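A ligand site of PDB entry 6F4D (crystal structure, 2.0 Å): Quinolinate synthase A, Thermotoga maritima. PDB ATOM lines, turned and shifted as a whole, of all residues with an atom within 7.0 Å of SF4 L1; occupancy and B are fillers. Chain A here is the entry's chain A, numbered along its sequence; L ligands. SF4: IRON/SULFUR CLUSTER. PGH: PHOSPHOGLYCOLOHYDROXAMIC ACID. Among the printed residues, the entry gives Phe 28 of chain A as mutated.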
ATOM      1  N   HIS A  26     -11.216   6.382   9.267  1.00  0.00           N
ATOM      2  CA  HIS A  26     -10.192   6.950   8.408  1.00  0.00           C
ATOM      3  C   HIS A  26     -10.167   8.500   8.546  1.00  0.00           C
ATOM      4  O   HIS A  26     -11.168   9.129   8.875  1.00  0.00           O
ATOM      5  CB  HIS A  26     -10.412   6.540   6.957  1.00  0.00           C
ATOM      6  CG  HIS A  26      -9.325   7.006   6.043  1.00  0.00           C
ATOM      7  ND1 HIS A  26      -9.403   8.190   5.343  1.00  0.00           N
ATOM      8  CD2 HIS A  26      -8.116   6.479   5.774  1.00  0.00           C
ATOM      9  CE1 HIS A  26      -8.289   8.362   4.655  1.00  0.00           C
ATOM     10  NE2 HIS A  26      -7.470   7.352   4.930  1.00  0.00           N
ATOM     11  N   PHE A  28     -10.391  10.829   6.487  1.00  0.00           N
ATOM     12  CA  PHE A  28     -11.261  11.592   5.608  1.00  0.00           C
ATOM     13  C   PHE A  28     -12.705  11.641   6.059  1.00  0.00           C
ATOM     14  O   PHE A  28     -13.535  12.289   5.403  1.00  0.00           O
ATOM     15  CB  PHE A  28     -11.217  11.051   4.181  1.00  0.00           C
ATOM     16  CG  PHE A  28      -9.880  11.165   3.532  1.00  0.00           C
ATOM     17  CD1 PHE A  28      -8.822  11.894   4.077  1.00  0.00           C
ATOM     18  CD2 PHE A  28      -9.680  10.552   2.311  1.00  0.00           C
ATOM     19  CE1 PHE A  28      -7.599  11.977   3.427  1.00  0.00           C
ATOM     20  CE2 PHE A  28      -8.473  10.627   1.662  1.00  0.00           C
ATOM     21  CZ  PHE A  28      -7.426  11.340   2.217  1.00  0.00           C
ATOM     22  N   VAL A  63     -14.226   3.556   3.719  1.00  0.00           N
ATOM     23  CA  VAL A  63     -14.795   2.949   2.492  1.00  0.00           C
ATOM     24  C   VAL A  63     -14.630   1.453   2.480  1.00  0.00           C
ATOM     25  O   VAL A  63     -13.798   0.912   3.215  1.00  0.00           O
ATOM     26  CB  VAL A  63     -14.301   3.581   1.190  1.00  0.00           C
ATOM     27  CG1 VAL A  63     -14.855   5.000   1.060  1.00  0.00           C
ATOM     28  CG2 VAL A  63     -12.785   3.554   1.096  1.00  0.00           C
ATOM     29  N   PHE A  65     -13.480  -1.158   0.880  1.00  0.00           N
ATOM     30  CA  PHE A  65     -12.280  -1.985   0.803  1.00  0.00           C
ATOM     31  C   PHE A  65     -11.511  -2.047   2.148  1.00  0.00           C
ATOM     32  O   PHE A  65     -10.919  -3.076   2.467  1.00  0.00           O
ATOM     33  CB  PHE A  65     -11.368  -1.559  -0.381  1.00  0.00           C
ATOM     34  CG  PHE A  65     -10.610  -0.295  -0.124  1.00  0.00           C
ATOM     35  CD1 PHE A  65      -9.505  -0.288   0.704  1.00  0.00           C
ATOM     36  CD2 PHE A  65     -11.005   0.895  -0.704  1.00  0.00           C
ATOM     37  CE1 PHE A  65      -8.792   0.889   0.945  1.00  0.00           C
ATOM     38  CE2 PHE A  65     -10.318   2.072  -0.452  1.00  0.00           C
ATOM     39  CZ  PHE A  65      -9.216   2.071   0.370  1.00  0.00           C
ATOM     40  N   THR A  87     -17.666   3.504  -1.127  1.00  0.00           N
ATOM     41  CA  THR A  87     -16.696   2.760  -1.935  1.00  0.00           C
ATOM     42  C   THR A  87     -15.653   3.708  -2.560  1.00  0.00           C
ATOM     43  O   THR A  87     -15.777   4.917  -2.434  1.00  0.00           O
ATOM     44  CB  THR A  87     -17.413   1.877  -3.006  1.00  0.00           C
ATOM     45  OG1 THR A  87     -16.495   0.924  -3.576  1.00  0.00           O
ATOM     46  CG2 THR A  87     -18.077   2.749  -4.106  1.00  0.00           C
ATOM     47  N   CYS A  88     -14.631   3.140  -3.168  1.00  0.00           N
ATOM     48  CA  CYS A  88     -13.557   3.900  -3.795  1.00  0.00           C
ATOM     49  C   CYS A  88     -13.692   3.658  -5.279  1.00  0.00           C
ATOM     50  O   CYS A  88     -13.402   2.568  -5.740  1.00  0.00           O
ATOM     51  CB  CYS A  88     -12.196   3.456  -3.277  1.00  0.00           C
ATOM     52  SG  CYS A  88     -10.848   4.298  -4.127  1.00  0.00           S
ATOM     53  N   PRO A  89     -14.189   4.656  -6.032  1.00  0.00           N
ATOM     54  CA  PRO A  89     -14.377   4.500  -7.476  1.00  0.00           C
ATOM     55  C   PRO A  89     -13.128   4.075  -8.289  1.00  0.00           C
ATOM     56  O   PRO A  89     -13.240   3.388  -9.304  1.00  0.00           O
ATOM     57  CB  PRO A  89     -14.881   5.892  -7.890  1.00  0.00           C
ATOM     58  CG  PRO A  89     -15.596   6.387  -6.676  1.00  0.00           C
ATOM     59  CD  PRO A  89     -14.719   5.955  -5.556  1.00  0.00           C
ATOM     60  N   MET A  90     -11.958   4.515  -7.829  1.00  0.00           N
ATOM     61  CA  MET A  90     -10.695   4.166  -8.462  1.00  0.00           C
ATOM     62  C   MET A  90     -10.434   2.657  -8.319  1.00  0.00           C
ATOM     63  O   MET A  90     -10.157   1.947  -9.302  1.00  0.00           O
ATOM     64  CB  MET A  90      -9.578   4.959  -7.793  1.00  0.00           C
ATOM     65  CG  MET A  90      -8.220   4.726  -8.417  1.00  0.00           C
ATOM     66  SD  MET A  90      -6.917   4.803  -7.204  1.00  0.00           S
ATOM     67  CE  MET A  90      -7.246   3.323  -6.272  1.00  0.00           C
ATOM     68  N   ALA A  91     -10.533   2.181  -7.079  1.00  0.00           N
ATOM     69  CA  ALA A  91     -10.408   0.804  -6.745  1.00  0.00           C
ATOM     70  C   ALA A  91     -11.282  -0.087  -7.606  1.00  0.00           C
ATOM     71  O   ALA A  91     -10.838  -1.122  -8.083  1.00  0.00           O
ATOM     72  CB  ALA A  91     -10.736   0.606  -5.277  1.00  0.00           C
ATOM     73  N   TYR A 114      -2.498  -1.856  -4.671  1.00  0.00           N
ATOM     74  CA  TYR A 114      -2.746  -0.827  -3.688  1.00  0.00           C
ATOM     75  C   TYR A 114      -3.909  -1.286  -2.811  1.00  0.00           C
ATOM     76  O   TYR A 114      -4.838  -1.947  -3.304  1.00  0.00           O
ATOM     77  CB  TYR A 114      -3.078   0.484  -4.410  1.00  0.00           C
ATOM     78  CG  TYR A 114      -3.127   1.734  -3.571  1.00  0.00           C
ATOM     79  CD1 TYR A 114      -2.260   1.938  -2.498  1.00  0.00           C
ATOM     80  CD2 TYR A 114      -4.006   2.779  -3.896  1.00  0.00           C
ATOM     81  CE1 TYR A 114      -2.295   3.101  -1.757  1.00  0.00           C
ATOM     82  CE2 TYR A 114      -4.059   3.949  -3.161  1.00  0.00           C
ATOM     83  CZ  TYR A 114      -3.206   4.121  -2.087  1.00  0.00           C
ATOM     84  OH  TYR A 114      -3.220   5.292  -1.331  1.00  0.00           O
ATOM     85  N   ASN A 116      -6.370   0.215  -1.854  1.00  0.00           N
ATOM     86  CA  ASN A 116      -7.607   0.609  -2.516  1.00  0.00           C
ATOM     87  C   ASN A 116      -7.831  -0.323  -3.711  1.00  0.00           C
ATOM     88  O   ASN A 116      -7.460  -0.026  -4.836  1.00  0.00           O
ATOM     89  CB  ASN A 116      -7.573   2.089  -2.962  1.00  0.00           C
ATOM     90  CG  ASN A 116      -7.328   3.066  -1.809  1.00  0.00           C
ATOM     91  OD1 ASN A 116      -6.351   2.944  -1.050  1.00  0.00           O
ATOM     92  ND2 ASN A 116      -8.204   4.061  -1.690  1.00  0.00           N
ATOM     93  N   ASP A 151      -3.901   2.441  -8.863  1.00  0.00           N
ATOM     94  CA  ASP A 151      -3.518   3.836  -8.971  1.00  0.00           C
ATOM     95  C   ASP A 151      -2.242   4.044  -9.803  1.00  0.00           C
ATOM     96  O   ASP A 151      -1.160   3.673  -9.383  1.00  0.00           O
ATOM     97  CB  ASP A 151      -3.345   4.436  -7.574  1.00  0.00           C
ATOM     98  CG  ASP A 151      -3.356   5.951  -7.595  1.00  0.00           C
ATOM     99  OD1 ASP A 151      -2.406   6.555  -8.117  1.00  0.00           O
ATOM    100  OD2 ASP A 151      -4.344   6.526  -7.089  1.00  0.00           O
ATOM    101  N   HIS A 174      -6.967   6.395 -11.373  1.00  0.00           N
ATOM    102  CA  HIS A 174      -6.551   7.588 -10.614  1.00  0.00           C
ATOM    103  C   HIS A 174      -7.647   8.025  -9.690  1.00  0.00           C
ATOM    104  O   HIS A 174      -8.824   7.749  -9.926  1.00  0.00           O
ATOM    105  CB  HIS A 174      -6.183   8.746 -11.550  1.00  0.00           C
ATOM    106  CG  HIS A 174      -7.355   9.369 -12.237  1.00  0.00           C
ATOM    107  ND1 HIS A 174      -7.751   8.997 -13.503  1.00  0.00           N
ATOM    108  CD2 HIS A 174      -8.231  10.311 -11.823  1.00  0.00           C
ATOM    109  CE1 HIS A 174      -8.823   9.700 -13.841  1.00  0.00           C
ATOM    110  NE2 HIS A 174      -9.136  10.500 -12.832  1.00  0.00           N
ATOM    111  N   CYS A 175      -7.247   8.741  -8.646  1.00  0.00           N
ATOM    112  CA  CYS A 175      -8.189   9.271  -7.683  1.00  0.00           C
ATOM    113  C   CYS A 175      -8.555  10.688  -8.098  1.00  0.00           C
ATOM    114  O   CYS A 175      -7.663  11.532  -8.150  1.00  0.00           O
ATOM    115  CB  CYS A 175      -7.550   9.301  -6.298  1.00  0.00           C
ATOM    116  SG  CYS A 175      -8.556  10.216  -5.153  1.00  0.00           S
ATOM    117  N   PRO A 176      -9.842  10.957  -8.405  1.00  0.00           N
ATOM    118  CA  PRO A 176     -10.267  12.312  -8.832  1.00  0.00           C
ATOM    119  C   PRO A 176     -10.127  13.393  -7.744  1.00  0.00           C
ATOM    120  O   PRO A 176      -9.874  14.551  -8.074  1.00  0.00           O
ATOM    121  CB  PRO A 176     -11.728  12.127  -9.232  1.00  0.00           C
ATOM    122  CG  PRO A 176     -12.169  10.891  -8.546  1.00  0.00           C
ATOM    123  CD  PRO A 176     -10.980  10.019  -8.355  1.00  0.00           C
ATOM    124  N   VAL A 177     -10.223  12.995  -6.475  1.00  0.00           N
ATOM    125  CA  VAL A 177     -10.044  13.889  -5.336  1.00  0.00           C
ATOM    126  C   VAL A 177      -8.644  14.509  -5.295  1.00  0.00           C
ATOM    127  O   VAL A 177      -8.499  15.656  -4.911  1.00  0.00           O
ATOM    128  CB  VAL A 177     -10.314  13.151  -3.994  1.00  0.00           C
ATOM    129  CG1 VAL A 177     -10.072  14.051  -2.794  1.00  0.00           C
ATOM    130  CG2 VAL A 177     -11.732  12.590  -3.966  1.00  0.00           C
ATOM    131  N   HIS A 178      -7.625  13.760  -5.711  1.00  0.00           N
ATOM    132  CA  HIS A 178      -6.235  14.197  -5.605  1.00  0.00           C
ATOM    133  C   HIS A 178      -5.702  14.816  -6.905  1.00  0.00           C
ATOM    134  O   HIS A 178      -4.506  15.083  -7.009  1.00  0.00           O
ATOM    135  CB  HIS A 178      -5.333  13.052  -5.132  1.00  0.00           C
ATOM    136  CG  HIS A 178      -5.481  12.767  -3.675  1.00  0.00           C
ATOM    137  ND1 HIS A 178      -6.393  11.864  -3.193  1.00  0.00           N
ATOM    138  CD2 HIS A 178      -4.858  13.295  -2.594  1.00  0.00           C
ATOM    139  CE1 HIS A 178      -6.317  11.837  -1.873  1.00  0.00           C
ATOM    140  NE2 HIS A 178      -5.393  12.697  -1.482  1.00  0.00           N
ATOM    141  N   GLU A 202      -0.932   9.850  -4.497  1.00  0.00           N
ATOM    142  CA  GLU A 202      -2.029   9.742  -5.457  1.00  0.00           C
ATOM    143  C   GLU A 202      -2.164  10.976  -6.347  1.00  0.00           C
ATOM    144  O   GLU A 202      -2.891  10.927  -7.319  1.00  0.00           O
ATOM    145  CB  GLU A 202      -3.382   9.490  -4.775  1.00  0.00           C
ATOM    146  CG  GLU A 202      -3.541   8.097  -4.166  1.00  0.00           C
ATOM    147  CD  GLU A 202      -4.783   7.984  -3.307  1.00  0.00           C
ATOM    148  OE1 GLU A 202      -5.755   8.710  -3.568  1.00  0.00           O
ATOM    149  OE2 GLU A 202      -4.791   7.215  -2.349  1.00  0.00           O
ATOM    150  N   THR A 236      -4.360  16.871   0.050  1.00  0.00           N
ATOM    151  CA  THR A 236      -5.144  15.666   0.190  1.00  0.00           C
ATOM    152  C   THR A 236      -6.587  16.056   0.502  1.00  0.00           C
ATOM    153  O   THR A 236      -6.953  17.255   0.398  1.00  0.00           O
ATOM    154  CB  THR A 236      -4.573  14.686   1.249  1.00  0.00           C
ATOM    155  OG1 THR A 236      -5.194  13.394   1.135  1.00  0.00           O
ATOM    156  CG2 THR A 236      -4.762  15.204   2.675  1.00  0.00           C
ATOM    157  N   GLU A 237      -7.398  15.076   0.874  1.00  0.00           N
ATOM    158  CA  GLU A 237      -8.816  15.284   1.061  1.00  0.00           C
ATOM    159  C   GLU A 237      -9.059  16.122   2.309  1.00  0.00           C
ATOM    160  O   GLU A 237      -8.297  16.013   3.307  1.00  0.00           O
ATOM    161  CB  GLU A 237      -9.540  13.957   1.122  1.00  0.00           C
ATOM    162  CG  GLU A 237     -11.021  13.964   0.733  1.00  0.00           C
ATOM    163  CD  GLU A 237     -11.958  14.202   1.888  1.00  0.00           C
ATOM    164  OE1 GLU A 237     -11.528  14.222   3.047  1.00  0.00           O
ATOM    165  OE2 GLU A 237     -13.156  14.395   1.627  1.00  0.00           O
ATOM    166  N   VAL A 260     -13.017  16.967  -1.871  1.00  0.00           N
ATOM    167  CA  VAL A 260     -13.932  16.200  -1.066  1.00  0.00           C
ATOM    168  C   VAL A 260     -14.124  14.807  -1.695  1.00  0.00           C
ATOM    169  O   VAL A 260     -14.307  14.696  -2.905  1.00  0.00           O
ATOM    170  CB  VAL A 260     -15.291  16.898  -0.952  1.00  0.00           C
ATOM    171  CG1 VAL A 260     -16.256  16.103  -0.063  1.00  0.00           C
ATOM    172  CG2 VAL A 260     -15.129  18.318  -0.411  1.00  0.00           C
ATOM    173  N   CYS A 261     -14.064  13.768  -0.871  1.00  0.00           N
ATOM    174  CA  CYS A 261     -14.365  12.409  -1.318  1.00  0.00           C
ATOM    175  C   CYS A 261     -15.807  12.168  -0.923  1.00  0.00           C
ATOM    176  O   CYS A 261     -16.114  11.958   0.267  1.00  0.00           O
ATOM    177  CB  CYS A 261     -13.451  11.345  -0.688  1.00  0.00           C
ATOM    178  SG  CYS A 261     -13.815   9.645  -1.238  1.00  0.00           S
ATOM    179  N   VAL A 262     -16.680  12.201  -1.930  1.00  0.00           N
ATOM    180  CA  VAL A 262     -18.106  12.067  -1.733  1.00  0.00           C
ATOM    181  C   VAL A 262     -18.422  10.760  -1.004  1.00  0.00           C
ATOM    182  O   VAL A 262     -19.296  10.709  -0.144  1.00  0.00           O
ATOM    183  CB  VAL A 262     -18.837  12.228  -3.095  1.00  0.00           C
ATOM    184  CG1 VAL A 262     -20.292  11.855  -3.006  1.00  0.00           C
ATOM    185  CG2 VAL A 262     -18.750  13.684  -3.526  1.00  0.00           C
ATOM    186  N   ASN A 263     -17.686   9.715  -1.332  1.00  0.00           N
ATOM    187  CA  ASN A 263     -17.871   8.445  -0.677  1.00  0.00           C
ATOM    188  C   ASN A 263     -17.511   8.444   0.793  1.00  0.00           C
ATOM    189  O   ASN A 263     -18.204   7.847   1.602  1.00  0.00           O
ATOM    190  CB  ASN A 263     -17.134   7.348  -1.425  1.00  0.00           C
ATOM    191  CG  ASN A 263     -17.943   6.797  -2.564  1.00  0.00           C
ATOM    192  OD1 ASN A 263     -18.848   5.980  -2.357  1.00  0.00           O
ATOM    193  ND2 ASN A 263     -17.589   7.170  -3.784  1.00  0.00           N
ATOM    194  N   MET A 264     -16.437   9.125   1.137  1.00  0.00           N
ATOM    195  CA  MET A 264     -16.056   9.242   2.528  1.00  0.00           C
ATOM    196  C   MET A 264     -17.077  10.018   3.363  1.00  0.00           C
ATOM    197  O   MET A 264     -17.247   9.740   4.566  1.00  0.00           O
ATOM    198  CB  MET A 264     -14.671   9.878   2.606  1.00  0.00           C
ATOM    199  CG  MET A 264     -13.551   8.935   2.209  1.00  0.00           C
ATOM    200  SD  MET A 264     -13.246   7.801   3.582  1.00  0.00           S
ATOM    201  CE  MET A 264     -11.607   7.196   3.168  1.00  0.00           C
HETATM  202 FE1  SF4 L   1      -9.688   8.962  -3.715  1.00  0.00          FE
HETATM  203 FE2  SF4 L   1     -11.869   8.592  -2.046  1.00  0.00          FE
HETATM  204 FE3  SF4 L   1      -9.195   7.689  -1.253  1.00  0.00          FE
HETATM  205 FE4  SF4 L   1     -10.701   6.436  -3.301  1.00  0.00          FE
HETATM  206  S1  SF4 L   1     -11.340   6.523  -1.141  1.00  0.00           S
HETATM  207  S2  SF4 L   1      -8.429   7.049  -3.374  1.00  0.00           S
HETATM  208  S3  SF4 L   1     -11.772   8.251  -4.370  1.00  0.00           S
HETATM  209  S4  SF4 L   1      -9.956   9.894  -1.646  1.00  0.00           S
HETATM  210  C1  PGH L   2      -6.587   7.698   0.499  1.00  0.00           C
HETATM  211  C2  PGH L   2      -5.367   8.045   1.297  1.00  0.00           C
HETATM  212  N2  PGH L   2      -6.909   8.652  -0.332  1.00  0.00           N
HETATM  213  O2  PGH L   2      -7.327   8.308  -1.595  1.00  0.00           O
HETATM  214  O1  PGH L   2      -7.137   6.605   0.558  1.00  0.00           O
HETATM  215  O1P PGH L   2      -4.789   6.882   1.875  1.00  0.00           O
HETATM  216  O2P PGH L   2      -2.833   7.956   2.850  1.00  0.00           O
HETATM  217  O3P PGH L   2      -3.561   5.601   3.511  1.00  0.00           O
HETATM  218  O4P PGH L   2      -4.946   7.606   4.208  1.00  0.00           O
HETATM  219  P   PGH L   2      -3.951   7.028   3.224  1.00  0.00           P
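FE1 of SF4 L1 is bound by SG of Cys 175 (2.2 Å). An iron atom (FE4) of SF4 L1 is bound by the side-chain sulfur (SG) of Cys 88 (2.3 Å). FE2 of SF4 L1 is bound by SG of Cys 261. ND2 of Asn 116 sits close to S2 of SF4 L1 (3.4 Å). OE2 of Glu 202 is in hydrogen-bond range of N2 of PGH L2. NE2 of His 26 is in hydrogen-bond range of O4P of PGH L2 (2.6 Å).
An iron atom (FE3) of SF4 L1 is bound by an oxygen (O2) of PGH L2.
The side-chain carboxylate (OE1) of Glu 202 lies close to the side-chain sulfur (SG) of Cys 175 (3.6 Å). N of Val 177 sits close to SG of Cys 175. The side-chain amide nitrogen (ND2) of Asn 116 lies close to the side-chain sulfur (SG) of Cys 88, at 3.6 Å. The side-chain sulfur (SG) of Cys 88 sits close to the backbone NH (N) of Ala 91, 3.6 Å away. The backbone NH of Met 264 sits close to the side-chain sulfur of Cys 261, 3.6 Å away. The side-chain carboxylate of Glu 202 is in hydrogen-bond range of a ring nitrogen (ND1) of His 178, at 3.2 Å. OE2 of Glu 202 is in hydrogen-bond range of OH of Tyr 114 (2.7 Å). A ring nitrogen (ND1) of His 26 lies within hydrogen-bond range of the backbone NH (N) of Phe 28 (3.0 Å).
A sulfur (S2) of SF4 L1 lies close to the side-chain carboxylate (OE1) of Glu 202 (3.2 Å). Phe 28 touches SF4 L1. Val 63 touches SF4 L1. Pro 89 touches SF4 L1 (CD to S3, 3.9 Å). CG2 of Val 177 touches S4 of SF4 L1, 3.98 Å away. Hydrophobic or aromatic side chains within 4 Å of SF4 L1: Phe 28, Val 63, Pro 89 and Val 177. Nine residues have an atom within 4 Å of SF4 L1: Phe 28, Val 63, Cys 88, Pro 89, Asn 116, Cys 175, Val 177, Glu 202 and Cys 261. The nearest printed residue that does not touch SF4 L1 is His 178 (4.1 Å).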
